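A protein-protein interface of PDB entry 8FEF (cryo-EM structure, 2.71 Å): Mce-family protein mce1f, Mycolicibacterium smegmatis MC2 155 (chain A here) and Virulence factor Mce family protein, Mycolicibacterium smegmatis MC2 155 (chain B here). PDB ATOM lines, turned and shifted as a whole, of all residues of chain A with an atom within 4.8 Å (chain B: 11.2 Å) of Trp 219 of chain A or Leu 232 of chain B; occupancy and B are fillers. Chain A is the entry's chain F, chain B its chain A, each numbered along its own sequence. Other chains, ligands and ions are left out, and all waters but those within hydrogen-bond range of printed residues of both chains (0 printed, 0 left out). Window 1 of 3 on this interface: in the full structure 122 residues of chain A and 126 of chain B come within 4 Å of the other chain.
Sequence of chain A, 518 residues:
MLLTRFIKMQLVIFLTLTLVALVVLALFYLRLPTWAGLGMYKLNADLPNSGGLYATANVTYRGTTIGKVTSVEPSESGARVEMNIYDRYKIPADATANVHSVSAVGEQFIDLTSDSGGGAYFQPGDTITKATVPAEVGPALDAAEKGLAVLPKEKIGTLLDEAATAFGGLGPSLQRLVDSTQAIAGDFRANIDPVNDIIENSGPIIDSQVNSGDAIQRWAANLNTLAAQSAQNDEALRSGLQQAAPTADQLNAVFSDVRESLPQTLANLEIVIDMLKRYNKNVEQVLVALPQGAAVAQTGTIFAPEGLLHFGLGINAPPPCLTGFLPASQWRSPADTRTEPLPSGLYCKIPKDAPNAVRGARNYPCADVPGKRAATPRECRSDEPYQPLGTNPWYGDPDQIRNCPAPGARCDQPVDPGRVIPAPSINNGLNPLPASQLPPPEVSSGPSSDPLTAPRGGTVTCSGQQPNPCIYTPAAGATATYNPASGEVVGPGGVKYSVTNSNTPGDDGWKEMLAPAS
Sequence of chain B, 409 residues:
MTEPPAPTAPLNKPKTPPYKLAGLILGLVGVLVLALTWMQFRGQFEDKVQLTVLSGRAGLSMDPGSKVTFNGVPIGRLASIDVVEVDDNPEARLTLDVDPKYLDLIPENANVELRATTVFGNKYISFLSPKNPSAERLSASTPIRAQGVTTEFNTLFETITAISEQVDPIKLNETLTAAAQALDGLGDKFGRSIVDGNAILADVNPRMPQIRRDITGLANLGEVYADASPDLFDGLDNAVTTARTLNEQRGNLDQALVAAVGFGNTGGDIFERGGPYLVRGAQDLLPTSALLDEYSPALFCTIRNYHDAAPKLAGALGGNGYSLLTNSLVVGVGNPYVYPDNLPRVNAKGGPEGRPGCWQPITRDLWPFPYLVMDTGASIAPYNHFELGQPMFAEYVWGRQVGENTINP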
ATOM      1  N   ALA A 215     -16.990  -9.203   3.517  1.00  0.00           N
ATOM      2  CA  ALA A 215     -16.635  -8.376   2.370  1.00  0.00           C
ATOM      3  C   ALA A 215     -17.866  -7.736   1.739  1.00  0.00           C
ATOM      4  O   ALA A 215     -17.831  -6.561   1.353  1.00  0.00           O
ATOM      5  CB  ALA A 215     -15.875  -9.207   1.337  1.00  0.00           C
ATOM      6  N   ILE A 216     -18.962  -8.491   1.610  1.00  0.00           N
ATOM      7  CA  ILE A 216     -20.147  -7.918   0.979  1.00  0.00           C
ATOM      8  C   ILE A 216     -20.783  -6.873   1.885  1.00  0.00           C
ATOM      9  O   ILE A 216     -21.270  -5.843   1.406  1.00  0.00           O
ATOM     10  CB  ILE A 216     -21.145  -9.005   0.528  1.00  0.00           C
ATOM     11  CG1 ILE A 216     -21.945  -9.598   1.682  1.00  0.00           C
ATOM     12  CG2 ILE A 216     -20.433 -10.102  -0.236  1.00  0.00           C
ATOM     13  CD1 ILE A 216     -23.053 -10.490   1.204  1.00  0.00           C
ATOM     14  N   GLN A 217     -20.768  -7.097   3.203  1.00  0.00           N
ATOM     15  CA  GLN A 217     -21.249  -6.062   4.114  1.00  0.00           C
ATOM     16  C   GLN A 217     -20.396  -4.804   4.011  1.00  0.00           C
ATOM     17  O   GLN A 217     -20.922  -3.683   4.005  1.00  0.00           O
ATOM     18  CB  GLN A 217     -21.266  -6.587   5.549  1.00  0.00           C
ATOM     19  CG  GLN A 217     -22.264  -7.703   5.785  1.00  0.00           C
ATOM     20  CD  GLN A 217     -22.257  -8.194   7.215  1.00  0.00           C
ATOM     21  OE1 GLN A 217     -21.593  -7.620   8.077  1.00  0.00           O
ATOM     22  NE2 GLN A 217     -22.998  -9.262   7.477  1.00  0.00           N
ATOM     23  N   ARG A 218     -19.075  -4.973   3.911  1.00  0.00           N
ATOM     24  CA  ARG A 218     -18.184  -3.822   3.828  1.00  0.00           C
ATOM     25  C   ARG A 218     -18.411  -3.032   2.546  1.00  0.00           C
ATOM     26  O   ARG A 218     -18.489  -1.797   2.577  1.00  0.00           O
ATOM     27  CB  ARG A 218     -16.728  -4.272   3.933  1.00  0.00           C
ATOM     28  CG  ARG A 218     -15.736  -3.124   3.946  1.00  0.00           C
ATOM     29  CD  ARG A 218     -16.097  -2.103   5.010  1.00  0.00           C
ATOM     30  NE  ARG A 218     -15.226  -0.935   4.968  1.00  0.00           N
ATOM     31  CZ  ARG A 218     -15.398   0.153   5.705  1.00  0.00           C
ATOM     32  NH1 ARG A 218     -16.411   0.262   6.549  1.00  0.00           N
ATOM     33  NH2 ARG A 218     -14.536   1.159   5.590  1.00  0.00           N
ATOM     34  N   TRP A 219     -18.522  -3.715   1.402  1.00  0.00           N
ATOM     35  CA  TRP A 219     -18.731  -2.942   0.182  1.00  0.00           C
ATOM     36  C   TRP A 219     -20.151  -2.406   0.084  1.00  0.00           C
ATOM     37  O   TRP A 219     -20.357  -1.392  -0.581  1.00  0.00           O
ATOM     38  CB  TRP A 219     -18.344  -3.719  -1.091  1.00  0.00           C
ATOM     39  CG  TRP A 219     -19.190  -4.891  -1.548  1.00  0.00           C
ATOM     40  CD1 TRP A 219     -18.811  -6.198  -1.554  1.00  0.00           C
ATOM     41  CD2 TRP A 219     -20.502  -4.856  -2.142  1.00  0.00           C
ATOM     42  NE1 TRP A 219     -19.810  -6.984  -2.072  1.00  0.00           N
ATOM     43  CE2 TRP A 219     -20.859  -6.186  -2.437  1.00  0.00           C
ATOM     44  CE3 TRP A 219     -21.413  -3.836  -2.436  1.00  0.00           C
ATOM     45  CZ2 TRP A 219     -22.085  -6.521  -3.007  1.00  0.00           C
ATOM     46  CZ3 TRP A 219     -22.630  -4.173  -2.996  1.00  0.00           C
ATOM     47  CH2 TRP A 219     -22.954  -5.503  -3.277  1.00  0.00           C
ATOM     48  N   ALA A 220     -21.127  -3.024   0.754  1.00  0.00           N
ATOM     49  CA  ALA A 220     -22.451  -2.415   0.833  1.00  0.00           C
ATOM     50  C   ALA A 220     -22.405  -1.108   1.615  1.00  0.00           C
ATOM     51  O   ALA A 220     -22.973  -0.095   1.188  1.00  0.00           O
ATOM     52  CB  ALA A 220     -23.441  -3.392   1.466  1.00  0.00           C
ATOM     53  N   ALA A 221     -21.713  -1.109   2.759  1.00  0.00           N
ATOM     54  CA  ALA A 221     -21.576   0.119   3.538  1.00  0.00           C
ATOM     55  C   ALA A 221     -20.809   1.187   2.766  1.00  0.00           C
ATOM     56  O   ALA A 221     -21.174   2.371   2.793  1.00  0.00           O
ATOM     57  CB  ALA A 221     -20.888  -0.181   4.869  1.00  0.00           C
ATOM     58  N   ASN A 222     -19.745   0.790   2.067  1.00  0.00           N
ATOM     59  CA  ASN A 222     -18.962   1.756   1.303  1.00  0.00           C
ATOM     60  C   ASN A 222     -19.739   2.286   0.103  1.00  0.00           C
ATOM     61  O   ASN A 222     -19.594   3.456  -0.265  1.00  0.00           O
ATOM     62  CB  ASN A 222     -17.646   1.132   0.861  1.00  0.00           C
ATOM     63  CG  ASN A 222     -16.697   0.910   2.011  1.00  0.00           C
ATOM     64  OD1 ASN A 222     -17.046   1.123   3.171  1.00  0.00           O
ATOM     65  ND2 ASN A 222     -15.486   0.477   1.697  1.00  0.00           N
ATOM     66  N   LEU A 223     -20.551   1.438  -0.530  1.00  0.00           N
ATOM     67  CA  LEU A 223     -21.431   1.905  -1.593  1.00  0.00           C
ATOM     68  C   LEU A 223     -22.426   2.919  -1.057  1.00  0.00           C
ATOM     69  O   LEU A 223     -22.678   3.945  -1.696  1.00  0.00           O
ATOM     70  CB  LEU A 223     -22.163   0.725  -2.230  1.00  0.00           C
ATOM     71  CG  LEU A 223     -23.255   1.066  -3.244  1.00  0.00           C
ATOM     72  CD1 LEU A 223     -22.650   1.631  -4.519  1.00  0.00           C
ATOM     73  CD2 LEU A 223     -24.112  -0.152  -3.542  1.00  0.00           C
ATOM     74  N   LEU B 221     -26.778 -17.353   4.195  1.00  0.00           N
ATOM     75  CA  LEU B 221     -26.761 -16.310   3.177  1.00  0.00           C
ATOM     76  C   LEU B 221     -27.918 -15.341   3.361  1.00  0.00           C
ATOM     77  O   LEU B 221     -27.765 -14.136   3.141  1.00  0.00           O
ATOM     78  CB  LEU B 221     -26.802 -16.935   1.784  1.00  0.00           C
ATOM     79  CG  LEU B 221     -26.693 -15.961   0.615  1.00  0.00           C
ATOM     80  CD1 LEU B 221     -25.480 -15.073   0.801  1.00  0.00           C
ATOM     81  CD2 LEU B 221     -26.611 -16.711  -0.698  1.00  0.00           C
ATOM     82  N   VAL B 224     -26.836 -13.027   6.131  1.00  0.00           N
ATOM     83  CA  VAL B 224     -25.833 -12.062   5.684  1.00  0.00           C
ATOM     84  C   VAL B 224     -26.472 -10.980   4.817  1.00  0.00           C
ATOM     85  O   VAL B 224     -26.181  -9.786   4.972  1.00  0.00           O
ATOM     86  CB  VAL B 224     -24.689 -12.780   4.945  1.00  0.00           C
ATOM     87  CG1 VAL B 224     -23.692 -11.775   4.446  1.00  0.00           C
ATOM     88  CG2 VAL B 224     -23.998 -13.763   5.871  1.00  0.00           C
ATOM     89  N   TYR B 225     -27.349 -11.380   3.893  1.00  0.00           N
ATOM     90  CA  TYR B 225     -28.020 -10.409   3.034  1.00  0.00           C
ATOM     91  C   TYR B 225     -28.932  -9.490   3.835  1.00  0.00           C
ATOM     92  O   TYR B 225     -29.008  -8.290   3.558  1.00  0.00           O
ATOM     93  CB  TYR B 225     -28.816 -11.129   1.945  1.00  0.00           C
ATOM     94  CG  TYR B 225     -27.988 -11.612   0.778  1.00  0.00           C
ATOM     95  CD1 TYR B 225     -26.704 -11.134   0.565  1.00  0.00           C
ATOM     96  CD2 TYR B 225     -28.497 -12.539  -0.120  1.00  0.00           C
ATOM     97  CE1 TYR B 225     -25.949 -11.572  -0.505  1.00  0.00           C
ATOM     98  CE2 TYR B 225     -27.749 -12.981  -1.193  1.00  0.00           C
ATOM     99  CZ  TYR B 225     -26.476 -12.494  -1.380  1.00  0.00           C
ATOM    100  OH  TYR B 225     -25.724 -12.929  -2.446  1.00  0.00           O
ATOM    101  N   ALA B 226     -29.649 -10.033   4.820  1.00  0.00           N
ATOM    102  CA  ALA B 226     -30.504  -9.199   5.655  1.00  0.00           C
ATOM    103  C   ALA B 226     -29.691  -8.236   6.510  1.00  0.00           C
ATOM    104  O   ALA B 226     -30.170  -7.146   6.837  1.00  0.00           O
ATOM    105  CB  ALA B 226     -31.393 -10.076   6.535  1.00  0.00           C
ATOM    106  N   ASP B 227     -28.469  -8.619   6.888  1.00  0.00           N
ATOM    107  CA  ASP B 227     -27.610  -7.688   7.612  1.00  0.00           C
ATOM    108  C   ASP B 227     -27.044  -6.610   6.696  1.00  0.00           C
ATOM    109  O   ASP B 227     -26.863  -5.467   7.131  1.00  0.00           O
ATOM    110  CB  ASP B 227     -26.476  -8.441   8.304  1.00  0.00           C
ATOM    111  CG  ASP B 227     -26.975  -9.385   9.380  1.00  0.00           C
ATOM    112  OD1 ASP B 227     -28.206  -9.493   9.553  1.00  0.00           O
ATOM    113  OD2 ASP B 227     -26.136 -10.020  10.052  1.00  0.00           O
ATOM    114  N   ALA B 228     -26.759  -6.942   5.439  1.00  0.00           N
ATOM    115  CA  ALA B 228     -26.113  -6.006   4.527  1.00  0.00           C
ATOM    116  C   ALA B 228     -27.086  -5.240   3.637  1.00  0.00           C
ATOM    117  O   ALA B 228     -26.645  -4.404   2.844  1.00  0.00           O
ATOM    118  CB  ALA B 228     -25.100  -6.743   3.647  1.00  0.00           C
ATOM    119  N   SER B 229     -28.386  -5.503   3.737  1.00  0.00           N
ATOM    120  CA  SER B 229     -29.348  -4.914   2.809  1.00  0.00           C
ATOM    121  C   SER B 229     -29.680  -3.435   3.025  1.00  0.00           C
ATOM    122  O   SER B 229     -29.811  -2.720   2.025  1.00  0.00           O
ATOM    123  CB  SER B 229     -30.642  -5.737   2.813  1.00  0.00           C
ATOM    124  OG  SER B 229     -31.035  -6.103   4.121  1.00  0.00           O
ATOM    125  N   PRO B 230     -29.879  -2.931   4.259  1.00  0.00           N
ATOM    126  CA  PRO B 230     -30.235  -1.503   4.382  1.00  0.00           C
ATOM    127  C   PRO B 230     -29.199  -0.563   3.787  1.00  0.00           C
ATOM    128  O   PRO B 230     -29.562   0.415   3.115  1.00  0.00           O
ATOM    129  CB  PRO B 230     -30.374  -1.306   5.897  1.00  0.00           C
ATOM    130  CG  PRO B 230     -30.683  -2.644   6.422  1.00  0.00           C
ATOM    131  CD  PRO B 230     -29.890  -3.584   5.582  1.00  0.00           C
ATOM    132  N   ASP B 231     -27.913  -0.848   4.004  1.00  0.00           N
ATOM    133  CA  ASP B 231     -26.864  -0.036   3.402  1.00  0.00           C
ATOM    134  C   ASP B 231     -26.908  -0.134   1.885  1.00  0.00           C
ATOM    135  O   ASP B 231     -26.753   0.875   1.185  1.00  0.00           O
ATOM    136  CB  ASP B 231     -25.498  -0.469   3.929  1.00  0.00           C
ATOM    137  CG  ASP B 231     -25.384  -0.331   5.431  1.00  0.00           C
ATOM    138  OD1 ASP B 231     -25.840   0.699   5.969  1.00  0.00           O
ATOM    139  OD2 ASP B 231     -24.844  -1.254   6.075  1.00  0.00           O
ATOM    140  N   LEU B 232     -27.127  -1.342   1.360  1.00  0.00           N
ATOM    141  CA  LEU B 232     -27.200  -1.521  -0.085  1.00  0.00           C
ATOM    142  C   LEU B 232     -28.338  -0.711  -0.685  1.00  0.00           C
ATOM    143  O   LEU B 232     -28.168  -0.069  -1.724  1.00  0.00           O
ATOM    144  CB  LEU B 232     -27.368  -2.999  -0.434  1.00  0.00           C
ATOM    145  CG  LEU B 232     -27.552  -3.250  -1.932  1.00  0.00           C
ATOM    146  CD1 LEU B 232     -26.234  -3.096  -2.673  1.00  0.00           C
ATOM    147  CD2 LEU B 232     -28.177  -4.605  -2.201  1.00  0.00           C
ATOM    148  N   PHE B 233     -29.499  -0.700  -0.032  1.00  0.00           N
ATOM    149  CA  PHE B 233     -30.643  -0.001  -0.606  1.00  0.00           C
ATOM    150  C   PHE B 233     -30.540   1.513  -0.451  1.00  0.00           C
ATOM    151  O   PHE B 233     -30.982   2.247  -1.343  1.00  0.00           O
ATOM    152  CB  PHE B 233     -31.942  -0.530  -0.004  1.00  0.00           C
ATOM    153  CG  PHE B 233     -32.378  -1.843  -0.590  1.00  0.00           C
ATOM    154  CD1 PHE B 233     -32.947  -1.894  -1.851  1.00  0.00           C
ATOM    155  CD2 PHE B 233     -32.211  -3.023   0.110  1.00  0.00           C
ATOM    156  CE1 PHE B 233     -33.342  -3.096  -2.399  1.00  0.00           C
ATOM    157  CE2 PHE B 233     -32.605  -4.229  -0.434  1.00  0.00           C
ATOM    158  CZ  PHE B 233     -33.172  -4.265  -1.689  1.00  0.00           C
ATOM    159  N   ASP B 234     -29.964   2.009   0.647  1.00  0.00           N
ATOM    160  CA  ASP B 234     -29.691   3.443   0.732  1.00  0.00           C
ATOM    161  C   ASP B 234     -28.691   3.871  -0.338  1.00  0.00           C
ATOM    162  O   ASP B 234     -28.867   4.913  -0.997  1.00  0.00           O
ATOM    163  CB  ASP B 234     -29.179   3.799   2.126  1.00  0.00           C
ATOM    164  CG  ASP B 234     -30.172   3.454   3.217  1.00  0.00           C
ATOM    165  OD1 ASP B 234     -31.257   2.931   2.890  1.00  0.00           O
ATOM    166  OD2 ASP B 234     -29.869   3.705   4.402  1.00  0.00           O
ATOM    167  N   GLY B 235     -27.637   3.073  -0.530  1.00  0.00           N
ATOM    168  CA  GLY B 235     -26.704   3.344  -1.605  1.00  0.00           C
ATOM    169  C   GLY B 235     -27.358   3.285  -2.968  1.00  0.00           C
ATOM    170  O   GLY B 235     -27.012   4.052  -3.860  1.00  0.00           O
ATOM    171  N   LEU B 236     -28.323   2.380  -3.142  1.00  0.00           N
ATOM    172  CA  LEU B 236     -29.032   2.292  -4.414  1.00  0.00           C
ATOM    173  C   LEU B 236     -29.928   3.504  -4.639  1.00  0.00           C
ATOM    174  O   LEU B 236     -30.074   3.960  -5.773  1.00  0.00           O
ATOM    175  CB  LEU B 236     -29.842   0.998  -4.486  1.00  0.00           C
ATOM    176  CG  LEU B 236     -29.051  -0.279  -4.779  1.00  0.00           C
ATOM    177  CD1 LEU B 236     -29.984  -1.470  -4.935  1.00  0.00           C
ATOM    178  CD2 LEU B 236     -28.184  -0.109  -6.016  1.00  0.00           C
ATOM    179  N   ASP B 237     -30.530   4.043  -3.576  1.00  0.00           N
ATOM    180  CA  ASP B 237     -31.311   5.274  -3.712  1.00  0.00           C
ATOM    181  C   ASP B 237     -30.434   6.435  -4.166  1.00  0.00           C
ATOM    182  O   ASP B 237     -30.749   7.138  -5.141  1.00  0.00           O
ATOM    183  CB  ASP B 237     -31.986   5.617  -2.385  1.00  0.00           C
ATOM    184  CG  ASP B 237     -33.390   5.072  -2.288  1.00  0.00           C
ATOM    185  OD1 ASP B 237     -34.137   5.173  -3.282  1.00  0.00           O
ATOM    186  OD2 ASP B 237     -33.751   4.542  -1.216  1.00  0.00           O
ATOM    187  N   ASN B 238     -29.321   6.654  -3.468  1.00  0.00           N
ATOM    188  CA  ASN B 238     -28.459   7.767  -3.850  1.00  0.00           C
ATOM    189  C   ASN B 238     -27.782   7.516  -5.198  1.00  0.00           C
ATOM    190  O   ASN B 238     -27.522   8.463  -5.957  1.00  0.00           O
ATOM    191  CB  ASN B 238     -27.443   8.027  -2.745  1.00  0.00           C
ATOM    192  CG  ASN B 238     -28.101   8.405  -1.432  1.00  0.00           C
ATOM    193  OD1 ASN B 238     -29.080   9.149  -1.407  1.00  0.00           O
ATOM    194  ND2 ASN B 238     -27.571   7.882  -0.333  1.00  0.00           N
ATOM    195  N   ALA B 239     -27.525   6.250  -5.529  1.00  0.00           N
ATOM    196  CA  ALA B 239     -27.002   5.905  -6.841  1.00  0.00           C
ATOM    197  C   ALA B 239     -28.044   6.121  -7.926  1.00  0.00           C
ATOM    198  O   ALA B 239     -27.687   6.444  -9.057  1.00  0.00           O
ATOM    199  CB  ALA B 239     -26.513   4.459  -6.846  1.00  0.00           C
ATOM    200  N   VAL B 240     -29.325   5.952  -7.601  1.00  0.00           N
ATOM    201  CA  VAL B 240     -30.394   6.304  -8.529  1.00  0.00           C
ATOM    202  C   VAL B 240     -30.383   7.799  -8.795  1.00  0.00           C
ATOM    203  O   VAL B 240     -30.535   8.243  -9.940  1.00  0.00           O
ATOM    204  CB  VAL B 240     -31.751   5.828  -7.977  1.00  0.00           C
ATOM    205  CG1 VAL B 240     -32.891   6.676  -8.514  1.00  0.00           C
ATOM    206  CG2 VAL B 240     -31.976   4.381  -8.335  1.00  0.00           C
ATOM    207  N   THR B 241     -30.195   8.597  -7.743  1.00  0.00           N
ATOM    208  CA  THR B 241     -30.087  10.046  -7.925  1.00  0.00           C
ATOM    209  C   THR B 241     -28.932  10.410  -8.861  1.00  0.00           C
ATOM    210  O   THR B 241     -29.117  11.125  -9.859  1.00  0.00           O
ATOM    211  CB  THR B 241     -29.917  10.734  -6.572  1.00  0.00           C
ATOM    212  OG1 THR B 241     -31.103  10.556  -5.788  1.00  0.00           O
ATOM    213  CG2 THR B 241     -29.659  12.219  -6.758  1.00  0.00           C
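OG of Ser 229 of chain B sits at hydrogen-bond distance from O of Tyr 225 of chain B (3.0 Å).
Of the printed residues of chain B, Gln 217 of chain A touches Val 224 (3.998 Å), Asp 227 (3.7 Å) and Ala 228 (3.7 Å). Trp 219 of chain A touches just one residue of chain B: Leu 232 (3.8 Å). Of the printed residues of chain B, Ala 221 of chain A touches Asp 231. Of the printed residues of chain B, Leu 223 of chain A touches Leu 232 (3.7 Å). Of the printed residues of chain A, Tyr 225 of chain B touches Ile 216 (3.5 Å). Of the printed residues of chain A, Asp 231 of chain B touches Ala 220 and Ala 221. Leu 232 of chain B touches just these residues of chain A: Trp 219 and Leu 223. The nearest residue of chain B that does not touch Trp 219 of chain A is Tyr 225 of chain B (6.8 Å). The nearest printed residue of chain B that does not touch Gln 217 of chain A is Asp 231 of chain B (5.1 Å).
Among the printed residues, merely in contact across the chains: Ile 216 of chain A with Val 224 of chain B, Ile 216 of chain A with Tyr 225 of chain B, Gln 217 of chain A with Val 224 of chain B, Gln 217 of chain A with Asp 227 of chain B, Gln 217 of chain A with Ala 228 of chain B, Trp 219 of chain A with Leu 232 of chain B, Ala 220 of chain A with Ala 228 of chain B, Ala 220 of chain A with Asp 231 of chain B, Ala 221 of chain A with Asp 231 of chain B and Leu 223 of chain A with Leu 232 of chain B.
Of the 19 printed residues of chain B, 6 touch a printed residue of chain A. Printed residues of chain B that touch a printed residue of chain A: Val 224, Tyr 225, Asp 227, Ala 228, Asp 231 and Leu 232. Hydrophobic or aromatic side chains of chain B within 4 Å of the printed part of chain A: Val 224, Tyr 225, Ala 228 and Leu 232. Of the 9 printed residues of chain A, 6 touch a printed residue of chain B. Hydrophobic or aromatic side chains of chain A within 4 Å of the printed part of chain B: Ile 216, Trp 219, Ala 220 and Leu 223. Among the printed residues, 10 pairs touch across the chains.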
